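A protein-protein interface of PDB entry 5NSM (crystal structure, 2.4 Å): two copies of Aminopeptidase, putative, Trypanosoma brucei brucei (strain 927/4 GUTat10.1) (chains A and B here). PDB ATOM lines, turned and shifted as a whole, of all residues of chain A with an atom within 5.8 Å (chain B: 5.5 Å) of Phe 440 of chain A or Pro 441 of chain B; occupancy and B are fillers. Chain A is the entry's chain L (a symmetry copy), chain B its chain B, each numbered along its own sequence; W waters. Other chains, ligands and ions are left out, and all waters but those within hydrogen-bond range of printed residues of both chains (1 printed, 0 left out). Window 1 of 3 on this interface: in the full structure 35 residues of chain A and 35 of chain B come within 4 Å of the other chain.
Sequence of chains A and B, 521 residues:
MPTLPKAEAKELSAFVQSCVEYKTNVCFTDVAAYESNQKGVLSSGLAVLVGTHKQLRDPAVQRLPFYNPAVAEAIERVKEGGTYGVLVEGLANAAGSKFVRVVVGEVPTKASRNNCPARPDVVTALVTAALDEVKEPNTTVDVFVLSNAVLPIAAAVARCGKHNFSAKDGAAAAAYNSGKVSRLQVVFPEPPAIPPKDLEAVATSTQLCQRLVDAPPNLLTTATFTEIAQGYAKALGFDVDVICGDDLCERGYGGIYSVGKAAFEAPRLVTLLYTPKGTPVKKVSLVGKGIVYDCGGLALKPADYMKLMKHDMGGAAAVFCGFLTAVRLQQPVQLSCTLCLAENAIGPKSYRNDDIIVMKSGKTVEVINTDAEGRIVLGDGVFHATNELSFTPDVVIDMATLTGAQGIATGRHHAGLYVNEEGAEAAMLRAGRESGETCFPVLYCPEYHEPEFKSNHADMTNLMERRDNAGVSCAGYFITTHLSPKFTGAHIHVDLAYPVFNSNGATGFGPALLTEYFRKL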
ATOM      1  N   ASN A 114       7.793 -30.335 -24.969  1.00  0.00           N
ATOM      2  CA  ASN A 114       8.458 -29.173 -24.323  1.00  0.00           C
ATOM      3  C   ASN A 114       8.292 -29.150 -22.826  1.00  0.00           C
ATOM      4  O   ASN A 114       8.631 -28.178 -22.167  1.00  0.00           O
ATOM      5  CB  ASN A 114       7.933 -27.871 -24.927  1.00  0.00           C
ATOM      6  CG  ASN A 114       8.260 -27.733 -26.389  1.00  0.00           C
ATOM      7  OD1 ASN A 114       7.365 -27.566 -27.170  1.00  0.00           O
ATOM      8  ND2 ASN A 114       9.528 -27.882 -26.774  1.00  0.00           N
ATOM      9  N   THR A 410       6.460 -17.008 -24.364  1.00  0.00           N
ATOM     10  CA  THR A 410       6.679 -18.391 -23.882  1.00  0.00           C
ATOM     11  C   THR A 410       5.872 -18.787 -22.642  1.00  0.00           C
ATOM     12  O   THR A 410       5.908 -19.924 -22.202  1.00  0.00           O
ATOM     13  CB  THR A 410       8.171 -18.690 -23.602  1.00  0.00           C
ATOM     14  OG1 THR A 410       8.652 -17.892 -22.539  1.00  0.00           O
ATOM     15  CG2 THR A 410       9.027 -18.436 -24.826  1.00  0.00           C
ATOM     16  N   HIS A 414       7.466 -21.434 -18.764  1.00  0.00           N
ATOM     17  CA  HIS A 414       8.668 -21.618 -19.603  1.00  0.00           C
ATOM     18  C   HIS A 414       9.464 -20.324 -19.674  1.00  0.00           C
ATOM     19  O   HIS A 414       9.002 -19.350 -20.252  1.00  0.00           O
ATOM     20  CB  HIS A 414       8.305 -22.075 -21.013  1.00  0.00           C
ATOM     21  CG  HIS A 414       7.825 -23.497 -21.103  1.00  0.00           C
ATOM     22  ND1 HIS A 414       6.557 -23.878 -20.731  1.00  0.00           N
ATOM     23  CD2 HIS A 414       8.439 -24.618 -21.555  1.00  0.00           C
ATOM     24  CE1 HIS A 414       6.418 -25.175 -20.925  1.00  0.00           C
ATOM     25  NE2 HIS A 414       7.538 -25.646 -21.441  1.00  0.00           N
ATOM     26  N   ALA A 415      10.663 -20.348 -19.122  1.00  0.00           N
ATOM     27  CA  ALA A 415      11.611 -19.250 -19.302  1.00  0.00           C
ATOM     28  C   ALA A 415      12.028 -19.169 -20.790  1.00  0.00           C
ATOM     29  O   ALA A 415      12.204 -20.194 -21.451  1.00  0.00           O
ATOM     30  CB  ALA A 415      12.833 -19.411 -18.432  1.00  0.00           C
ATOM     31  N   GLY A 416      12.184 -17.948 -21.285  1.00  0.00           N
ATOM     32  CA  GLY A 416      12.617 -17.752 -22.658  1.00  0.00           C
ATOM     33  C   GLY A 416      14.129 -17.846 -22.769  1.00  0.00           C
ATOM     34  O   GLY A 416      14.839 -17.260 -21.970  1.00  0.00           O
ATOM     35  N   LEU A 417      14.603 -18.549 -23.776  1.00  0.00           N
ATOM     36  CA  LEU A 417      16.067 -18.683 -24.037  1.00  0.00           C
ATOM     37  C   LEU A 417      16.521 -18.005 -25.327  1.00  0.00           C
ATOM     38  O   LEU A 417      16.039 -18.299 -26.401  1.00  0.00           O
ATOM     39  CB  LEU A 417      16.492 -20.141 -24.154  1.00  0.00           C
ATOM     40  CG  LEU A 417      16.254 -21.037 -22.961  1.00  0.00           C
ATOM     41  CD1 LEU A 417      16.820 -22.412 -23.299  1.00  0.00           C
ATOM     42  CD2 LEU A 417      16.862 -20.499 -21.679  1.00  0.00           C
ATOM     43  N   LEU A 429      17.795 -26.490 -22.690  1.00  0.00           N
ATOM     44  CA  LEU A 429      16.429 -27.083 -22.882  1.00  0.00           C
ATOM     45  C   LEU A 429      16.295 -28.452 -22.216  1.00  0.00           C
ATOM     46  O   LEU A 429      15.319 -28.712 -21.509  1.00  0.00           O
ATOM     47  CB  LEU A 429      16.030 -27.202 -24.340  1.00  0.00           C
ATOM     48  CG  LEU A 429      15.776 -25.856 -25.006  1.00  0.00           C
ATOM     49  CD1 LEU A 429      15.721 -26.009 -26.515  1.00  0.00           C
ATOM     50  CD2 LEU A 429      14.507 -25.197 -24.474  1.00  0.00           C
ATOM     51  N   THR A 438      11.315 -25.658 -16.729  1.00  0.00           N
ATOM     52  CA  THR A 438      11.277 -25.709 -18.187  1.00  0.00           C
ATOM     53  C   THR A 438      11.566 -24.356 -18.854  1.00  0.00           C
ATOM     54  O   THR A 438      11.257 -23.275 -18.306  1.00  0.00           O
ATOM     55  CB  THR A 438       9.913 -26.191 -18.687  1.00  0.00           C
ATOM     56  OG1 THR A 438       8.885 -25.476 -17.995  1.00  0.00           O
ATOM     57  CG2 THR A 438       9.745 -27.648 -18.428  1.00  0.00           C
ATOM     58  N   CYS A 439      12.128 -24.471 -20.041  1.00  0.00           N
ATOM     59  CA  CYS A 439      12.531 -23.351 -20.876  1.00  0.00           C
ATOM     60  C   CYS A 439      12.003 -23.526 -22.298  1.00  0.00           C
ATOM     61  O   CYS A 439      11.561 -24.584 -22.676  1.00  0.00           O
ATOM     62  CB  CYS A 439      14.023 -23.247 -20.919  1.00  0.00           C
ATOM     63  SG  CYS A 439      14.757 -22.838 -19.330  1.00  0.00           S
ATOM     64  N   PHE A 440      12.030 -22.459 -23.062  1.00  0.00           N
ATOM     65  CA  PHE A 440      11.701 -22.533 -24.485  1.00  0.00           C
ATOM     66  C   PHE A 440      12.464 -21.441 -25.241  1.00  0.00           C
ATOM     67  O   PHE A 440      12.611 -20.346 -24.740  1.00  0.00           O
ATOM     68  CB  PHE A 440      10.190 -22.406 -24.733  1.00  0.00           C
ATOM     69  CG  PHE A 440       9.784 -22.773 -26.131  1.00  0.00           C
ATOM     70  CD1 PHE A 440       9.630 -24.124 -26.493  1.00  0.00           C
ATOM     71  CD2 PHE A 440       9.635 -21.799 -27.104  1.00  0.00           C
ATOM     72  CE1 PHE A 440       9.310 -24.473 -27.810  1.00  0.00           C
ATOM     73  CE2 PHE A 440       9.307 -22.146 -28.405  1.00  0.00           C
ATOM     74  CZ  PHE A 440       9.138 -23.476 -28.764  1.00  0.00           C
ATOM     75  N   PRO A 441      12.958 -21.742 -26.462  1.00  0.00           N
ATOM     76  CA  PRO A 441      13.743 -20.718 -27.135  1.00  0.00           C
ATOM     77  C   PRO A 441      12.924 -19.572 -27.694  1.00  0.00           C
ATOM     78  O   PRO A 441      11.790 -19.741 -28.121  1.00  0.00           O
ATOM     79  CB  PRO A 441      14.424 -21.466 -28.290  1.00  0.00           C
ATOM     80  CG  PRO A 441      13.882 -22.847 -28.323  1.00  0.00           C
ATOM     81  CD  PRO A 441      12.892 -23.004 -27.222  1.00  0.00           C
ATOM     82  N   VAL A 442      13.542 -18.408 -27.678  1.00  0.00           N
ATOM     83  CA  VAL A 442      13.057 -17.282 -28.471  1.00  0.00           C
ATOM     84  C   VAL A 442      14.014 -17.021 -29.639  1.00  0.00           C
ATOM     85  O   VAL A 442      15.171 -17.440 -29.631  1.00  0.00           O
ATOM     86  CB  VAL A 442      12.812 -16.003 -27.658  1.00  0.00           C
ATOM     87  CG1 VAL A 442      11.745 -16.279 -26.614  1.00  0.00           C
ATOM     88  CG2 VAL A 442      14.081 -15.486 -27.008  1.00  0.00           C
ATOM     89  N   THR B 410       7.974 -13.456 -32.028  1.00  0.00           N
ATOM     90  CA  THR B 410       8.921 -13.834 -33.126  1.00  0.00           C
ATOM     91  C   THR B 410       9.284 -12.712 -34.117  1.00  0.00           C
ATOM     92  O   THR B 410      10.094 -12.895 -35.010  1.00  0.00           O
ATOM     93  CB  THR B 410       8.415 -15.051 -33.934  1.00  0.00           C
ATOM     94  OG1 THR B 410       7.214 -14.716 -34.624  1.00  0.00           O
ATOM     95  CG2 THR B 410       8.153 -16.228 -33.036  1.00  0.00           C
ATOM     96  N   ALA B 415       7.415 -15.647 -39.176  1.00  0.00           N
ATOM     97  CA  ALA B 415       6.076 -16.171 -38.819  1.00  0.00           C
ATOM     98  C   ALA B 415       6.225 -17.166 -37.671  1.00  0.00           C
ATOM     99  O   ALA B 415       7.200 -17.918 -37.602  1.00  0.00           O
ATOM    100  CB  ALA B 415       5.399 -16.836 -39.999  1.00  0.00           C
ATOM    101  N   GLY B 416       5.273 -17.144 -36.763  1.00  0.00           N
ATOM    102  CA  GLY B 416       5.306 -18.061 -35.616  1.00  0.00           C
ATOM    103  C   GLY B 416       4.688 -19.393 -35.977  1.00  0.00           C
ATOM    104  O   GLY B 416       3.662 -19.447 -36.626  1.00  0.00           O
ATOM    105  N   LEU B 417       5.349 -20.464 -35.579  1.00  0.00           N
ATOM    106  CA  LEU B 417       4.864 -21.829 -35.849  1.00  0.00           C
ATOM    107  C   LEU B 417       4.438 -22.530 -34.577  1.00  0.00           C
ATOM    108  O   LEU B 417       5.233 -22.766 -33.682  1.00  0.00           O
ATOM    109  CB  LEU B 417       5.932 -22.705 -36.523  1.00  0.00           C
ATOM    110  CG  LEU B 417       6.467 -22.247 -37.868  1.00  0.00           C
ATOM    111  CD1 LEU B 417       7.464 -23.295 -38.379  1.00  0.00           C
ATOM    112  CD2 LEU B 417       5.363 -22.026 -38.900  1.00  0.00           C
ATOM    113  N   GLU B 425       7.328 -29.585 -38.122  1.00  0.00           N
ATOM    114  CA  GLU B 425       7.873 -28.292 -37.708  1.00  0.00           C
ATOM    115  C   GLU B 425       9.252 -28.026 -38.324  1.00  0.00           C
ATOM    116  O   GLU B 425       9.503 -26.970 -38.871  1.00  0.00           O
ATOM    117  CB  GLU B 425       7.974 -28.198 -36.174  1.00  0.00           C
ATOM    118  CG  GLU B 425       8.440 -26.843 -35.655  1.00  0.00           C
ATOM    119  CD  GLU B 425       8.606 -26.834 -34.152  1.00  0.00           C
ATOM    120  OE1 GLU B 425       7.612 -26.585 -33.451  1.00  0.00           O
ATOM    121  OE2 GLU B 425       9.719 -27.074 -33.668  1.00  0.00           O
ATOM    122  N   LEU B 429      10.278 -25.111 -41.001  1.00  0.00           N
ATOM    123  CA  LEU B 429      11.436 -24.245 -40.704  1.00  0.00           C
ATOM    124  C   LEU B 429      12.473 -24.250 -41.821  1.00  0.00           C
ATOM    125  O   LEU B 429      12.939 -23.197 -42.250  1.00  0.00           O
ATOM    126  CB  LEU B 429      12.130 -24.613 -39.386  1.00  0.00           C
ATOM    127  CG  LEU B 429      11.325 -24.260 -38.135  1.00  0.00           C
ATOM    128  CD1 LEU B 429      11.914 -24.945 -36.911  1.00  0.00           C
ATOM    129  CD2 LEU B 429      11.213 -22.739 -37.928  1.00  0.00           C
ATOM    130  N   CYS B 439      10.438 -18.506 -40.627  1.00  0.00           N
ATOM    131  CA  CYS B 439       9.534 -18.886 -39.572  1.00  0.00           C
ATOM    132  C   CYS B 439      10.329 -19.150 -38.294  1.00  0.00           C
ATOM    133  O   CYS B 439      11.533 -19.290 -38.326  1.00  0.00           O
ATOM    134  CB  CYS B 439       8.774 -20.141 -39.937  1.00  0.00           C
ATOM    135  SG  CYS B 439       7.644 -19.919 -41.319  1.00  0.00           S
ATOM    136  N   PHE B 440       9.628 -19.190 -37.164  1.00  0.00           N
ATOM    137  CA  PHE B 440      10.254 -19.583 -35.904  1.00  0.00           C
ATOM    138  C   PHE B 440       9.223 -20.227 -35.029  1.00  0.00           C
ATOM    139  O   PHE B 440       8.070 -19.786 -35.000  1.00  0.00           O
ATOM    140  CB  PHE B 440      10.915 -18.383 -35.210  1.00  0.00           C
ATOM    141  CG  PHE B 440      11.819 -18.766 -34.087  1.00  0.00           C
ATOM    142  CD1 PHE B 440      13.115 -19.221 -34.331  1.00  0.00           C
ATOM    143  CD2 PHE B 440      11.346 -18.783 -32.792  1.00  0.00           C
ATOM    144  CE1 PHE B 440      13.930 -19.650 -33.287  1.00  0.00           C
ATOM    145  CE2 PHE B 440      12.143 -19.180 -31.755  1.00  0.00           C
ATOM    146  CZ  PHE B 440      13.442 -19.612 -31.995  1.00  0.00           C
ATOM    147  N   PRO B 441       9.597 -21.287 -34.310  1.00  0.00           N
ATOM    148  CA  PRO B 441       8.552 -21.913 -33.473  1.00  0.00           C
ATOM    149  C   PRO B 441       8.102 -21.119 -32.253  1.00  0.00           C
ATOM    150  O   PRO B 441       8.893 -20.429 -31.626  1.00  0.00           O
ATOM    151  CB  PRO B 441       9.178 -23.251 -33.003  1.00  0.00           C
ATOM    152  CG  PRO B 441      10.585 -23.228 -33.446  1.00  0.00           C
ATOM    153  CD  PRO B 441      10.890 -21.952 -34.167  1.00  0.00           C
ATOM    154  N   VAL B 442       6.835 -21.290 -31.922  1.00  0.00           N
ATOM    155  CA  VAL B 442       6.344 -20.892 -30.603  1.00  0.00           C
ATOM    156  C   VAL B 442       6.024 -22.138 -29.782  1.00  0.00           C
ATOM    157  O   VAL B 442       5.829 -23.222 -30.307  1.00  0.00           O
ATOM    158  CB  VAL B 442       5.152 -19.920 -30.661  1.00  0.00           C
ATOM    159  CG1 VAL B 442       5.577 -18.637 -31.360  1.00  0.00           C
ATOM    160  CG2 VAL B 442       3.954 -20.533 -31.349  1.00  0.00           C
ATOM    161  N   LEU B 443       5.973 -21.935 -28.475  1.00  0.00           N
ATOM    162  CA  LEU B 443       5.732 -23.005 -27.510  1.00  0.00           C
ATOM    163  C   LEU B 443       4.534 -23.876 -27.897  1.00  0.00           C
ATOM    164  O   LEU B 443       3.432 -23.360 -28.127  1.00  0.00           O
ATOM    165  CB  LEU B 443       5.512 -22.443 -26.121  1.00  0.00           C
ATOM    166  CG  LEU B 443       5.161 -23.462 -25.032  1.00  0.00           C
ATOM    167  CD1 LEU B 443       6.357 -24.345 -24.700  1.00  0.00           C
ATOM    168  CD2 LEU B 443       4.642 -22.765 -23.784  1.00  0.00           C
ATOM    169  N   TYR B 444       4.777 -25.191 -27.988  1.00  0.00           N
ATOM    170  CA  TYR B 444       3.695 -26.186 -28.100  1.00  0.00           C
ATOM    171  C   TYR B 444       3.583 -26.909 -26.767  1.00  0.00           C
ATOM    172  O   TYR B 444       4.448 -27.699 -26.403  1.00  0.00           O
ATOM    173  CB  TYR B 444       3.914 -27.197 -29.229  1.00  0.00           C
ATOM    174  CG  TYR B 444       2.775 -28.198 -29.392  1.00  0.00           C
ATOM    175  CD1 TYR B 444       1.617 -27.863 -30.091  1.00  0.00           C
ATOM    176  CD2 TYR B 444       2.852 -29.488 -28.819  1.00  0.00           C
ATOM    177  CE1 TYR B 444       0.573 -28.765 -30.239  1.00  0.00           C
ATOM    178  CE2 TYR B 444       1.809 -30.406 -28.975  1.00  0.00           C
ATOM    179  CZ  TYR B 444       0.680 -30.037 -29.702  1.00  0.00           C
ATOM    180  OH  TYR B 444      -0.383 -30.920 -29.845  1.00  0.00           O
HETATM  181  O   HOH W   1       9.599 -18.753 -29.546  1.00  0.00           O
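Water W1 bridges the backbone carbonyl oxygen (O) of Pro 441 of chain B and the backbone carbonyl oxygen (O) of Pro 441 of chain A.
The backbone NH (N) of Val 442 of chain A is in hydrogen-bond range of the backbone carbonyl oxygen (O) of Leu 417 of chain A, 2.8 Å away. O of Phe 440 of chain B lies within hydrogen-bond range of N of Leu 417 of chain B, at 2.9 Å. O of His 414 of chain A lies within hydrogen-bond range of OG1 of Thr 410 of chain A (2.7 Å). The backbone carbonyl oxygen (O) of Asn 114 of chain A sits at hydrogen-bond distance from a ring nitrogen (NE2) of His 414 of chain A, 2.9 Å away. The backbone carbonyl oxygen (O) of Phe 440 of chain A sits at hydrogen-bond distance from the backbone NH (N) of Leu 417 of chain A (2.9 Å). The backbone carbonyl oxygen of Ala 415 of chain B lies within hydrogen-bond range of the backbone NH of Phe 440 of chain B.
Pro 441 of chain B touches just one residue of chain A: Phe 440. Of the printed residues of chain B, Val 442 of chain A touches Phe 440. Of the printed residues of chain B, His 414 of chain A touches Leu 443 (3.7 Å). Ala 415 of chain B touches none of the printed residues of chain A. The nearest residue of chain B that does not touch Phe 440 of chain A is Tyr 444 of chain B (4.6 Å). The nearest residue of chain A that does not touch Pro 441 of chain B is Pro 441 of chain A (4.6 Å).
Printed residues of chain B that touch a printed residue of chain A: Phe 440, Pro 441, Val 442, Leu 443 and Tyr 444. Hydrophobic or aromatic side chains of chain B that line the printed part of chain A: Phe 440 and Leu 443. Among the printed residues, no Asp or Glu carboxylate lies within 4 Å of a Lys or Arg side-chain nitrogen of the other chain.
Phe 440 of chain A touches Pro 441 of chain B, and with the chains exchanged Pro 441 of chain A touches Phe 440 of chain B. Phe 440 of chain A touches Val 442 of chain B, and with the chains exchanged Val 442 of chain A touches Phe 440 of chain B. 9 positions are printed for both chains.
The backbone carbonyl oxygen of Tyr 444 of chain B lies close to the side-chain amide oxygen of Asn 114 of chain A (3.0 Å).
Leu 443 of chain B touches Asn 114 of chain A. CD2 of Leu 443 of chain B touches O of Thr 410 of chain A, at 3.5 Å. CD1 of Leu 443 of chain B touches NE2 of His 414 of chain A (3.7 Å). Phe 440 of chain A touches Pro 441 of chain B (CE2 to O, 3.7 Å). Phe 440 of chain A touches Val 442 of chain B (CZ to C, 3.5 Å). Phe 440 of chain A touches Leu 443 of chain B (CE2 to N, 3.3 Å). O of Pro 441 of chain A touches CE2 of Phe 440 of chain B, at 3.7 Å. C of Val 442 of chain A touches CZ of Phe 440 of chain B, at 3.5 Å.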
